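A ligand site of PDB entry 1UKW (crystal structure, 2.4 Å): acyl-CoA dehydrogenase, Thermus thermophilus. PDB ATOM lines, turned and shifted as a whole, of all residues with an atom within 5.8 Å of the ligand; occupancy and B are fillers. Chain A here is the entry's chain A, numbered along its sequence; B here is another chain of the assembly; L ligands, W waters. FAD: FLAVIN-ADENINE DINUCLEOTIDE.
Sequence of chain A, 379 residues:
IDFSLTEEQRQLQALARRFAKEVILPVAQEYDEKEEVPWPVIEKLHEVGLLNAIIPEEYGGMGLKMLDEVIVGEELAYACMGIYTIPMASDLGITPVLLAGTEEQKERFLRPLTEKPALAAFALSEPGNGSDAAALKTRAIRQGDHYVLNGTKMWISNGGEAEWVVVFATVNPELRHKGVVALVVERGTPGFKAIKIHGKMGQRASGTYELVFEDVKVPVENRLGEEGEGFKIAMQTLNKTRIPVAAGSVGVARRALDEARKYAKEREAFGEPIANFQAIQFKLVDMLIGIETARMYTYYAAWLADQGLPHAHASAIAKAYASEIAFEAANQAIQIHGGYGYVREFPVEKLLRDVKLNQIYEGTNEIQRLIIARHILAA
Water W4 lies within hydrogen-bond range of O2P of the ligand (2.5 Å), NE1 of Trp 155 (2.9 Å), O of Glu 126 (3.0 Å) and O of Pro 127 (3.4 Å).
Water W1 lies within hydrogen-bond range of N of Phe 122, O of Ser 157 and O4 of the ligand.
Merely in contact with the ligand: Asn 129 (3.95 Å), Ile 156 (3.7 Å), Lys 200 (3.9 Å), Thr 208 (3.9 Å), Leu 357 (3.3 Å), Ile 360 (3.3 Å), Tyr 361 (3.5 Å), Gly 363 (3.8 Å) and Leu 370 (3.5 Å).
Hydrophobic or aromatic side chains within 4 Å of the ligand: Phe 122, Leu 124, Trp 155, Leu 357, Ile 360, Tyr 361 and Leu 370.
Of the 31 residues printed, 20 come within 4 Å of the ligand.
The nearest printed residue that does not touch the ligand is Ala 123 (4.1 Å).
A nitrogen (N5) of the ligand lies close to the backbone carbonyl oxygen (O) of Trp 155.
O2A of the ligand sits at hydrogen-bond distance from OG of Ser 131 (2.5 Å).
O2B of the ligand is in hydrogen-bond range of OG1 of Thr 364.
The side-chain carboxylate (OE2) of Glu 366 is in hydrogen-bond range of an oxygen (O2B) of the ligand (2.8 Å).
The backbone carbonyl oxygen (O) of Phe 122 is in hydrogen-bond range of a nitrogen (N3) of the ligand, 2.8 Å away.
The backbone NH (N) of Ser 125 sits at hydrogen-bond distance from an oxygen (O2) of the ligand, 3.1 Å away.
O3' of the ligand lies within hydrogen-bond range of OG of Ser 125, 2.8 Å away.
An oxygen (O2') of the ligand is in hydrogen-bond range of the backbone NH of Glu 362.
The backbone NH of Ser 157 sits at hydrogen-bond distance from an oxygen (O4) of the ligand (2.8 Å).
N5 of the ligand sits at hydrogen-bond distance from OG of Ser 157 (3.0 Å).
The side-chain amide nitrogen (NE2) of Gln 278 of chain B lies within hydrogen-bond range of a nitrogen (N1A) of the ligand (2.8 Å).
O2 of the ligand sits at hydrogen-bond distance from N of Leu 124.
N of Gly 130 lies within hydrogen-bond range of O2P of the ligand, at 3.5 Å.
O3' of the ligand sits at hydrogen-bond distance from O of Gly 130.
OG1 of Thr 364 lies close to N of Ile 367, 3.4 Å away.
O of Ser 125 lies within hydrogen-bond range of N of Met 154.
The side-chain hydroxyl (OG1) of Thr 208 lies within hydrogen-bond range of the side-chain amino group (NZ) of Lys 200 (2.9 Å).
The backbone carbonyl oxygen of Asp 132 is in hydrogen-bond range of the side-chain amide nitrogen of Asn 129 (2.8 Å).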
ATOM      1  N   ALA A  89      21.117  28.119  -2.204  1.00  0.00           N
ATOM      2  CA  ALA A  89      21.608  27.603  -3.484  1.00  0.00           C
ATOM      3  C   ALA A  89      22.116  28.730  -4.378  1.00  0.00           C
ATOM      4  O   ALA A  89      22.970  28.516  -5.228  1.00  0.00           O
ATOM      5  CB  ALA A  89      20.514  26.808  -4.198  1.00  0.00           C
ATOM      6  N   LEU A  92      25.358  29.332  -3.355  1.00  0.00           N
ATOM      7  CA  LEU A  92      26.138  28.231  -3.896  1.00  0.00           C
ATOM      8  C   LEU A  92      26.584  28.552  -5.317  1.00  0.00           C
ATOM      9  O   LEU A  92      27.723  28.257  -5.702  1.00  0.00           O
ATOM     10  CB  LEU A  92      25.312  26.937  -3.898  1.00  0.00           C
ATOM     11  CG  LEU A  92      25.917  25.706  -4.587  1.00  0.00           C
ATOM     12  CD1 LEU A  92      27.167  25.242  -3.857  1.00  0.00           C
ATOM     13  CD2 LEU A  92      24.893  24.599  -4.623  1.00  0.00           C
ATOM     14  N   PHE A 122      24.103  26.449  -9.390  1.00  0.00           N
ATOM     15  CA  PHE A 122      25.276  25.588  -9.385  1.00  0.00           C
ATOM     16  C   PHE A 122      24.887  24.240  -9.998  1.00  0.00           C
ATOM     17  O   PHE A 122      24.071  23.502  -9.437  1.00  0.00           O
ATOM     18  CB  PHE A 122      25.723  25.409  -7.934  1.00  0.00           C
ATOM     19  CG  PHE A 122      26.981  24.598  -7.762  1.00  0.00           C
ATOM     20  CD1 PHE A 122      28.216  25.233  -7.646  1.00  0.00           C
ATOM     21  CD2 PHE A 122      26.918  23.212  -7.649  1.00  0.00           C
ATOM     22  CE1 PHE A 122      29.370  24.492  -7.412  1.00  0.00           C
ATOM     23  CE2 PHE A 122      28.072  22.468  -7.429  1.00  0.00           C
ATOM     24  CZ  PHE A 122      29.298  23.108  -7.300  1.00  0.00           C
ATOM     25  N   ALA A 123      25.469  23.905 -11.144  1.00  0.00           N
ATOM     26  CA  ALA A 123      25.164  22.652 -11.826  1.00  0.00           C
ATOM     27  C   ALA A 123      26.360  21.713 -11.961  1.00  0.00           C
ATOM     28  O   ALA A 123      27.223  21.899 -12.821  1.00  0.00           O
ATOM     29  CB  ALA A 123      24.557  22.940 -13.212  1.00  0.00           C
ATOM     30  N   LEU A 124      26.390  20.686 -11.119  1.00  0.00           N
ATOM     31  CA  LEU A 124      27.468  19.706 -11.126  1.00  0.00           C
ATOM     32  C   LEU A 124      26.916  18.307 -11.384  1.00  0.00           C
ATOM     33  O   LEU A 124      27.441  17.561 -12.204  1.00  0.00           O
ATOM     34  CB  LEU A 124      28.205  19.731  -9.784  1.00  0.00           C
ATOM     35  CG  LEU A 124      29.292  18.693  -9.595  1.00  0.00           C
ATOM     36  CD1 LEU A 124      30.374  18.908 -10.625  1.00  0.00           C
ATOM     37  CD2 LEU A 124      29.876  18.796  -8.193  1.00  0.00           C
ATOM     38  N   SER A 125      25.843  17.955 -10.681  1.00  0.00           N
ATOM     39  CA  SER A 125      25.217  16.633 -10.806  1.00  0.00           C
ATOM     40  C   SER A 125      24.625  16.387 -12.191  1.00  0.00           C
ATOM     41  O   SER A 125      24.237  17.307 -12.902  1.00  0.00           O
ATOM     42  CB  SER A 125      24.121  16.464  -9.753  1.00  0.00           C
ATOM     43  OG  SER A 125      24.642  16.535  -8.428  1.00  0.00           O
ATOM     44  N   GLU A 126      24.545  15.121 -12.570  1.00  0.00           N
ATOM     45  CA  GLU A 126      23.977  14.763 -13.853  1.00  0.00           C
ATOM     46  C   GLU A 126      23.078  13.551 -13.628  1.00  0.00           C
ATOM     47  O   GLU A 126      23.161  12.895 -12.595  1.00  0.00           O
ATOM     48  CB  GLU A 126      25.092  14.437 -14.852  1.00  0.00           C
ATOM     49  CG  GLU A 126      26.148  15.538 -14.985  1.00  0.00           C
ATOM     50  CD  GLU A 126      27.117  15.313 -16.146  1.00  0.00           C
ATOM     51  OE1 GLU A 126      27.561  14.156 -16.349  1.00  0.00           O
ATOM     52  OE2 GLU A 126      27.431  16.291 -16.862  1.00  0.00           O
ATOM     53  N   PRO A 127      22.200  13.255 -14.590  1.00  0.00           N
ATOM     54  CA  PRO A 127      21.290  12.109 -14.445  1.00  0.00           C
ATOM     55  C   PRO A 127      21.978  10.807 -14.006  1.00  0.00           C
ATOM     56  O   PRO A 127      21.507  10.139 -13.089  1.00  0.00           O
ATOM     57  CB  PRO A 127      20.674  11.992 -15.835  1.00  0.00           C
ATOM     58  CG  PRO A 127      20.605  13.412 -16.290  1.00  0.00           C
ATOM     59  CD  PRO A 127      21.965  13.951 -15.863  1.00  0.00           C
ATOM     60  N   GLY A 128      23.085  10.461 -14.655  1.00  0.00           N
ATOM     61  CA  GLY A 128      23.763   9.228 -14.305  1.00  0.00           C
ATOM     62  C   GLY A 128      24.934   9.371 -13.375  1.00  0.00           C
ATOM     63  O   GLY A 128      25.768   8.469 -13.283  1.00  0.00           O
ATOM     64  N   ASN A 129      24.999  10.482 -12.649  1.00  0.00           N
ATOM     65  CA  ASN A 129      26.120  10.704 -11.751  1.00  0.00           C
ATOM     66  C   ASN A 129      25.923  11.913 -10.850  1.00  0.00           C
ATOM     67  O   ASN A 129      25.582  13.005 -11.312  1.00  0.00           O
ATOM     68  CB  ASN A 129      27.393  10.861 -12.582  1.00  0.00           C
ATOM     69  CG  ASN A 129      28.547  11.413 -11.783  1.00  0.00           C
ATOM     70  OD1 ASN A 129      29.045  10.756 -10.863  1.00  0.00           O
ATOM     71  ND2 ASN A 129      28.956  12.641 -12.106  1.00  0.00           N
ATOM     72  N   GLY A 130      26.139  11.715  -9.551  1.00  0.00           N
ATOM     73  CA  GLY A 130      25.986  12.806  -8.605  1.00  0.00           C
ATOM     74  C   GLY A 130      27.072  12.764  -7.540  1.00  0.00           C
ATOM     75  O   GLY A 130      27.616  13.792  -7.155  1.00  0.00           O
ATOM     76  N   SER A 131      27.399  11.560  -7.079  1.00  0.00           N
ATOM     77  CA  SER A 131      28.431  11.404  -6.064  1.00  0.00           C
ATOM     78  C   SER A 131      29.786  11.351  -6.725  1.00  0.00           C
ATOM     79  O   SER A 131      30.757  11.934  -6.229  1.00  0.00           O
ATOM     80  CB  SER A 131      28.217  10.111  -5.265  1.00  0.00           C
ATOM     81  OG  SER A 131      27.025  10.188  -4.511  1.00  0.00           O
ATOM     82  N   ASP A 132      29.858  10.647  -7.853  1.00  0.00           N
ATOM     83  CA  ASP A 132      31.098  10.546  -8.592  1.00  0.00           C
ATOM     84  C   ASP A 132      31.224  11.770  -9.479  1.00  0.00           C
ATOM     85  O   ASP A 132      31.142  11.680 -10.711  1.00  0.00           O
ATOM     86  CB  ASP A 132      31.106   9.279  -9.448  1.00  0.00           C
ATOM     87  CG  ASP A 132      32.399   9.122 -10.223  1.00  0.00           C
ATOM     88  OD1 ASP A 132      33.379   9.831  -9.886  1.00  0.00           O
ATOM     89  OD2 ASP A 132      32.432   8.285 -11.150  1.00  0.00           O
ATOM     90  N   MET A 154      21.428  17.469 -13.683  1.00  0.00           N
ATOM     91  CA  MET A 154      20.263  17.029 -12.942  1.00  0.00           C
ATOM     92  C   MET A 154      20.142  17.547 -11.509  1.00  0.00           C
ATOM     93  O   MET A 154      21.125  17.689 -10.797  1.00  0.00           O
ATOM     94  CB  MET A 154      20.204  15.495 -12.961  1.00  0.00           C
ATOM     95  CG  MET A 154      18.913  14.915 -12.402  1.00  0.00           C
ATOM     96  SD  MET A 154      17.469  15.589 -13.231  1.00  0.00           S
ATOM     97  CE  MET A 154      16.166  14.522 -12.561  1.00  0.00           C
ATOM     98  N   TRP A 155      18.897  17.801 -11.108  1.00  0.00           N
ATOM     99  CA  TRP A 155      18.593  18.289  -9.772  1.00  0.00           C
ATOM    100  C   TRP A 155      19.117  19.704  -9.541  1.00  0.00           C
ATOM    101  O   TRP A 155      19.412  20.039  -8.415  1.00  0.00           O
ATOM    102  CB  TRP A 155      19.241  17.405  -8.708  1.00  0.00           C
ATOM    103  CG  TRP A 155      19.021  15.933  -8.854  1.00  0.00           C
ATOM    104  CD1 TRP A 155      19.996  14.989  -9.041  1.00  0.00           C
ATOM    105  CD2 TRP A 155      17.776  15.235  -8.845  1.00  0.00           C
ATOM    106  NE1 TRP A 155      19.430  13.749  -9.142  1.00  0.00           N
ATOM    107  CE2 TRP A 155      18.062  13.863  -9.035  1.00  0.00           C
ATOM    108  CE3 TRP A 155      16.441  15.628  -8.696  1.00  0.00           C
ATOM    109  CZ2 TRP A 155      17.064  12.878  -9.074  1.00  0.00           C
ATOM    110  CZ3 TRP A 155      15.434  14.650  -8.744  1.00  0.00           C
ATOM    111  CH2 TRP A 155      15.763  13.295  -8.932  1.00  0.00           C
ATOM    112  N   ILE A 156      19.218  20.541 -10.570  1.00  0.00           N
ATOM    113  CA  ILE A 156      19.752  21.878 -10.344  1.00  0.00           C
ATOM    114  C   ILE A 156      18.812  22.843  -9.615  1.00  0.00           C
ATOM    115  O   ILE A 156      17.730  23.154 -10.105  1.00  0.00           O
ATOM    116  CB  ILE A 156      20.188  22.532 -11.687  1.00  0.00           C
ATOM    117  CG1 ILE A 156      21.025  21.527 -12.512  1.00  0.00           C
ATOM    118  CG2 ILE A 156      20.996  23.800 -11.429  1.00  0.00           C
ATOM    119  CD1 ILE A 156      22.138  20.858 -11.729  1.00  0.00           C
ATOM    120  N   SER A 157      19.222  23.299  -8.441  1.00  0.00           N
ATOM    121  CA  SER A 157      18.428  24.236  -7.646  1.00  0.00           C
ATOM    122  C   SER A 157      18.479  25.620  -8.301  1.00  0.00           C
ATOM    123  O   SER A 157      19.570  26.079  -8.667  1.00  0.00           O
ATOM    124  CB  SER A 157      18.972  24.343  -6.223  1.00  0.00           C
ATOM    125  OG  SER A 157      18.918  23.103  -5.540  1.00  0.00           O
ATOM    126  N   LYS A 200       8.435  16.497  -5.564  1.00  0.00           N
ATOM    127  CA  LYS A 200       9.440  16.290  -4.532  1.00  0.00           C
ATOM    128  C   LYS A 200       8.759  16.009  -3.200  1.00  0.00           C
ATOM    129  O   LYS A 200       7.654  16.477  -2.961  1.00  0.00           O
ATOM    130  CB  LYS A 200      10.346  17.519  -4.399  1.00  0.00           C
ATOM    131  CG  LYS A 200      11.232  17.760  -5.589  1.00  0.00           C
ATOM    132  CD  LYS A 200      12.389  18.686  -5.253  1.00  0.00           C
ATOM    133  CE  LYS A 200      11.909  20.010  -4.687  1.00  0.00           C
ATOM    134  NZ  LYS A 200      13.032  20.904  -4.346  1.00  0.00           N
ATOM    135  N   THR A 208      13.651  22.886  -8.631  1.00  0.00           N
ATOM    136  CA  THR A 208      14.735  21.989  -8.978  1.00  0.00           C
ATOM    137  C   THR A 208      14.557  21.662 -10.450  1.00  0.00           C
ATOM    138  O   THR A 208      13.450  21.366 -10.902  1.00  0.00           O
ATOM    139  CB  THR A 208      14.697  20.737  -8.121  1.00  0.00           C
ATOM    140  OG1 THR A 208      14.570  21.117  -6.747  1.00  0.00           O
ATOM    141  CG2 THR A 208      15.980  19.927  -8.306  1.00  0.00           C
ATOM    142  N   LEU A 357      16.151  15.862   2.707  1.00  0.00           N
ATOM    143  CA  LEU A 357      16.948  16.284   1.557  1.00  0.00           C
ATOM    144  C   LEU A 357      18.329  16.753   2.006  1.00  0.00           C
ATOM    145  O   LEU A 357      19.308  16.585   1.279  1.00  0.00           O
ATOM    146  CB  LEU A 357      16.266  17.431   0.826  1.00  0.00           C
ATOM    147  CG  LEU A 357      16.420  17.576  -0.696  1.00  0.00           C
ATOM    148  CD1 LEU A 357      16.327  19.060  -1.030  1.00  0.00           C
ATOM    149  CD2 LEU A 357      17.758  17.010  -1.191  1.00  0.00           C
ATOM    150  N   ILE A 360      21.046  14.393   1.587  1.00  0.00           N
ATOM    151  CA  ILE A 360      21.342  13.920   0.246  1.00  0.00           C
ATOM    152  C   ILE A 360      22.035  14.916  -0.677  1.00  0.00           C
ATOM    153  O   ILE A 360      23.040  14.564  -1.293  1.00  0.00           O
ATOM    154  CB  ILE A 360      20.053  13.428  -0.442  1.00  0.00           C
ATOM    155  CG1 ILE A 360      19.519  12.229   0.335  1.00  0.00           C
ATOM    156  CG2 ILE A 360      20.335  13.071  -1.894  1.00  0.00           C
ATOM    157  CD1 ILE A 360      18.117  11.839  -0.064  1.00  0.00           C
ATOM    158  N   TYR A 361      21.524  16.143  -0.792  1.00  0.00           N
ATOM    159  CA  TYR A 361      22.172  17.100  -1.695  1.00  0.00           C
ATOM    160  C   TYR A 361      23.432  17.745  -1.144  1.00  0.00           C
ATOM    161  O   TYR A 361      23.665  17.753   0.059  1.00  0.00           O
ATOM    162  CB  TYR A 361      21.172  18.153  -2.218  1.00  0.00           C
ATOM    163  CG  TYR A 361      20.619  19.185  -1.244  1.00  0.00           C
ATOM    164  CD1 TYR A 361      20.838  19.107   0.128  1.00  0.00           C
ATOM    165  CD2 TYR A 361      19.840  20.237  -1.728  1.00  0.00           C
ATOM    166  CE1 TYR A 361      20.285  20.045   0.998  1.00  0.00           C
ATOM    167  CE2 TYR A 361      19.287  21.175  -0.880  1.00  0.00           C
ATOM    168  CZ  TYR A 361      19.505  21.080   0.483  1.00  0.00           C
ATOM    169  OH  TYR A 361      18.941  22.011   1.326  1.00  0.00           O
ATOM    170  N   GLU A 362      24.228  18.273  -2.061  1.00  0.00           N
ATOM    171  CA  GLU A 362      25.518  18.885  -1.738  1.00  0.00           C
ATOM    172  C   GLU A 362      26.411  17.795  -1.141  1.00  0.00           C
ATOM    173  O   GLU A 362      27.267  18.063  -0.296  1.00  0.00           O
ATOM    174  CB  GLU A 362      25.368  20.079  -0.773  1.00  0.00           C
ATOM    175  CG  GLU A 362      25.275  21.423  -1.515  1.00  0.00           C
ATOM    176  CD  GLU A 362      25.420  22.635  -0.608  1.00  0.00           C
ATOM    177  OE1 GLU A 362      26.476  22.786   0.047  1.00  0.00           O
ATOM    178  OE2 GLU A 362      24.483  23.458  -0.569  1.00  0.00           O
ATOM    179  N   GLY A 363      26.196  16.565  -1.602  1.00  0.00           N
ATOM    180  CA  GLY A 363      26.964  15.424  -1.141  1.00  0.00           C
ATOM    181  C   GLY A 363      26.162  14.616  -0.142  1.00  0.00           C
ATOM    182  O   GLY A 363      25.698  15.159   0.861  1.00  0.00           O
ATOM    183  N   THR A 364      25.976  13.326  -0.406  1.00  0.00           N
ATOM    184  CA  THR A 364      25.213  12.496   0.517  1.00  0.00           C
ATOM    185  C   THR A 364      26.027  12.319   1.773  1.00  0.00           C
ATOM    186  O   THR A 364      27.255  12.473   1.769  1.00  0.00           O
ATOM    187  CB  THR A 364      24.916  11.087  -0.041  1.00  0.00           C
ATOM    188  OG1 THR A 364      26.141  10.435  -0.387  1.00  0.00           O
ATOM    189  CG2 THR A 364      24.009  11.163  -1.255  1.00  0.00           C
ATOM    190  N   ASN A 365      25.355  12.003   2.864  1.00  0.00           N
ATOM    191  CA  ASN A 365      26.055  11.800   4.109  1.00  0.00           C
ATOM    192  C   ASN A 365      27.051  10.637   4.036  1.00  0.00           C
ATOM    193  O   ASN A 365      27.990  10.593   4.831  1.00  0.00           O
ATOM    194  CB  ASN A 365      25.050  11.647   5.244  1.00  0.00           C
ATOM    195  CG  ASN A 365      24.330  12.954   5.546  1.00  0.00           C
ATOM    196  OD1 ASN A 365      24.649  13.989   4.961  1.00  0.00           O
ATOM    197  ND2 ASN A 365      23.362  12.907   6.446  1.00  0.00           N
ATOM    198  N   GLU A 366      26.863   9.728   3.077  1.00  0.00           N
ATOM    199  CA  GLU A 366      27.795   8.605   2.919  1.00  0.00           C
ATOM    200  C   GLU A 366      29.106   9.106   2.356  1.00  0.00           C
ATOM    201  O   GLU A 366      30.176   8.690   2.792  1.00  0.00           O
ATOM    202  CB  GLU A 366      27.252   7.519   1.988  1.00  0.00           C
ATOM    203  CG  GLU A 366      26.250   6.591   2.629  1.00  0.00           C
ATOM    204  CD  GLU A 366      24.942   7.295   2.894  1.00  0.00           C
ATOM    205  OE1 GLU A 366      24.289   6.960   3.909  1.00  0.00           O
ATOM    206  OE2 GLU A 366      24.559   8.162   2.089  1.00  0.00           O
ATOM    207  N   ILE A 367      29.039   9.981   1.355  1.00  0.00           N
ATOM    208  CA  ILE A 367      30.281  10.491   0.791  1.00  0.00           C
ATOM    209  C   ILE A 367      30.867  11.526   1.744  1.00  0.00           C
ATOM    210  O   ILE A 367      32.085  11.754   1.732  1.00  0.00           O
ATOM    211  CB  ILE A 367      30.091  11.043  -0.653  1.00  0.00           C
ATOM    212  CG1 ILE A 367      29.433  12.405  -0.644  1.00  0.00           C
ATOM    213  CG2 ILE A 367      29.313  10.022  -1.502  1.00  0.00           C
ATOM    214  CD1 ILE A 367      30.437  13.528  -0.546  1.00  0.00           C
ATOM    215  N   LEU A 370      32.911   9.470   3.539  1.00  0.00           N
ATOM    216  CA  LEU A 370      34.051   9.054   2.733  1.00  0.00           C
ATOM    217  C   LEU A 370      35.105  10.166   2.796  1.00  0.00           C
ATOM    218  O   LEU A 370      36.301   9.901   2.846  1.00  0.00           O
ATOM    219  CB  LEU A 370      33.612   8.812   1.283  1.00  0.00           C
ATOM    220  CG  LEU A 370      33.397   7.351   0.873  1.00  0.00           C
ATOM    221  CD1 LEU A 370      32.826   6.554   2.020  1.00  0.00           C
ATOM    222  CD2 LEU A 370      32.474   7.302  -0.337  1.00  0.00           C
ATOM    223  N   GLN B 278      35.137  -0.250   3.856  1.00  0.00           N
ATOM    224  CA  GLN B 278      34.207   0.818   4.144  1.00  0.00           C
ATOM    225  C   GLN B 278      33.483   0.686   5.481  1.00  0.00           C
ATOM    226  O   GLN B 278      33.213   1.682   6.133  1.00  0.00           O
ATOM    227  CB  GLN B 278      33.192   0.937   3.000  1.00  0.00           C
ATOM    228  CG  GLN B 278      32.759   2.360   2.687  1.00  0.00           C
ATOM    229  CD  GLN B 278      31.934   2.448   1.407  1.00  0.00           C
ATOM    230  OE1 GLN B 278      30.791   1.995   1.356  1.00  0.00           O
ATOM    231  NE2 GLN B 278      32.510   3.054   0.366  1.00  0.00           N
ATOM    232  N   PHE B 282      33.803   3.714   8.200  1.00  0.00           N
ATOM    233  CA  PHE B 282      32.637   4.380   8.771  1.00  0.00           C
ATOM    234  C   PHE B 282      32.616   4.331  10.295  1.00  0.00           C
ATOM    235  O   PHE B 282      32.115   5.252  10.925  1.00  0.00           O
ATOM    236  CB  PHE B 282      31.362   3.778   8.184  1.00  0.00           C
ATOM    237  CG  PHE B 282      30.983   4.366   6.868  1.00  0.00           C
ATOM    238  CD1 PHE B 282      31.948   4.621   5.894  1.00  0.00           C
ATOM    239  CD2 PHE B 282      29.662   4.730   6.610  1.00  0.00           C
ATOM    240  CE1 PHE B 282      31.611   5.234   4.694  1.00  0.00           C
ATOM    241  CE2 PHE B 282      29.314   5.336   5.406  1.00  0.00           C
ATOM    242  CZ  PHE B 282      30.289   5.594   4.446  1.00  0.00           C
HETATM  243  PA  FAD L   1      24.196   8.335  -6.383  1.00  0.00           P
HETATM  244  O1A FAD L   1      24.060   7.263  -7.409  1.00  0.00           O
HETATM  245  O2A FAD L   1      25.578   8.724  -5.998  1.00  0.00           O
HETATM  246  O5B FAD L   1      23.467   7.908  -5.084  1.00  0.00           O
HETATM  247  C5B FAD L   1      24.197   6.887  -4.476  1.00  0.00           C
HETATM  248  C4B FAD L   1      23.704   6.335  -3.187  1.00  0.00           C
HETATM  249  O4B FAD L   1      24.820   5.443  -3.023  1.00  0.00           O
HETATM  250  C3B FAD L   1      23.800   7.343  -2.028  1.00  0.00           C
HETATM  251  O3B FAD L   1      22.974   6.840  -0.955  1.00  0.00           O
HETATM  252  C2B FAD L   1      25.196   7.347  -1.690  1.00  0.00           C
HETATM  253  O2B FAD L   1      25.612   7.783  -0.436  1.00  0.00           O
HETATM  254  C1B FAD L   1      25.686   5.902  -1.957  1.00  0.00           C
HETATM  255  N9A FAD L   1      27.012   5.878  -2.494  1.00  0.00           N
HETATM  256  C8A FAD L   1      27.507   6.375  -3.742  1.00  0.00           C
HETATM  257  N7A FAD L   1      28.779   6.206  -3.918  1.00  0.00           N
HETATM  258  C5A FAD L   1      29.204   5.560  -2.762  1.00  0.00           C
HETATM  259  C6A FAD L   1      30.462   5.111  -2.327  1.00  0.00           C
HETATM  260  N6A FAD L   1      31.560   5.254  -3.067  1.00  0.00           N
HETATM  261  N1A FAD L   1      30.536   4.494  -1.083  1.00  0.00           N
HETATM  262  C2A FAD L   1      29.436   4.343  -0.303  1.00  0.00           C
HETATM  263  N3A FAD L   1      28.144   4.768  -0.662  1.00  0.00           N
HETATM  264  C4A FAD L   1      28.190   5.371  -1.949  1.00  0.00           C
HETATM  265  N1  FAD L   1      23.602  18.950  -7.308  1.00  0.00           N
HETATM  266  C2  FAD L   1      24.204  20.076  -7.848  1.00  0.00           C
HETATM  267  O2  FAD L   1      25.334  20.013  -8.374  1.00  0.00           O
HETATM  268  N3  FAD L   1      23.527  21.285  -7.783  1.00  0.00           N
HETATM  269  C4  FAD L   1      22.232  21.485  -7.222  1.00  0.00           C
HETATM  270  O4  FAD L   1      21.710  22.640  -7.240  1.00  0.00           O
HETATM  271  C4X FAD L   1      21.647  20.331  -6.718  1.00  0.00           C
HETATM  272  N5  FAD L   1      20.327  20.480  -6.186  1.00  0.00           N
HETATM  273  C5X FAD L   1      19.688  19.296  -5.701  1.00  0.00           C
HETATM  274  C6  FAD L   1      18.370  19.374  -5.227  1.00  0.00           C
HETATM  275  C7  FAD L   1      17.637  18.243  -4.757  1.00  0.00           C
HETATM  276  C7M FAD L   1      16.192  18.430  -4.293  1.00  0.00           C
HETATM  277  C8  FAD L   1      18.294  16.954  -4.774  1.00  0.00           C
HETATM  278  C8M FAD L   1      17.596  15.688  -4.314  1.00  0.00           C
HETATM  279  C9  FAD L   1      19.617  16.831  -5.226  1.00  0.00           C
HETATM  280  C9A FAD L   1      20.338  17.954  -5.701  1.00  0.00           C
HETATM  281  N10 FAD L   1      21.736  17.940  -6.249  1.00  0.00           N
HETATM  282  C10 FAD L   1      22.340  19.083  -6.757  1.00  0.00           C
HETATM  283  C1' FAD L   1      22.469  16.691  -6.273  1.00  0.00           C
HETATM  284  C2' FAD L   1      23.234  16.286  -4.979  1.00  0.00           C
HETATM  285  O2' FAD L   1      24.205  17.330  -4.721  1.00  0.00           O
HETATM  286  C3' FAD L   1      24.000  14.971  -5.124  1.00  0.00           C
HETATM  287  O3' FAD L   1      25.063  15.043  -6.071  1.00  0.00           O
HETATM  288  C4' FAD L   1      23.108  13.892  -5.596  1.00  0.00           C
HETATM  289  O4' FAD L   1      22.023  13.724  -4.632  1.00  0.00           O
HETATM  290  C5' FAD L   1      23.700  12.597  -5.959  1.00  0.00           C
HETATM  291  O5' FAD L   1      22.542  11.910  -6.320  1.00  0.00           O
HETATM  292  P   FAD L   1      22.419  10.645  -7.129  1.00  0.00           P
HETATM  293  O1P FAD L   1      21.007  10.238  -7.076  1.00  0.00           O
HETATM  294  O2P FAD L   1      22.893  11.208  -8.413  1.00  0.00           O
HETATM  295  O3P FAD L   1      23.552   9.549  -7.078  1.00  0.00           O
HETATM  296  O   HOH W   1      22.170  25.541  -7.789  1.00  0.00           O
HETATM  297  O   HOH W   2      27.027   8.975  -8.824  1.00  0.00           O
HETATM  298  O   HOH W   3      25.116  20.240  -5.062  1.00  0.00           O
HETATM  299  O   HOH W   4      21.411  12.011 -10.293  1.00  0.00           O
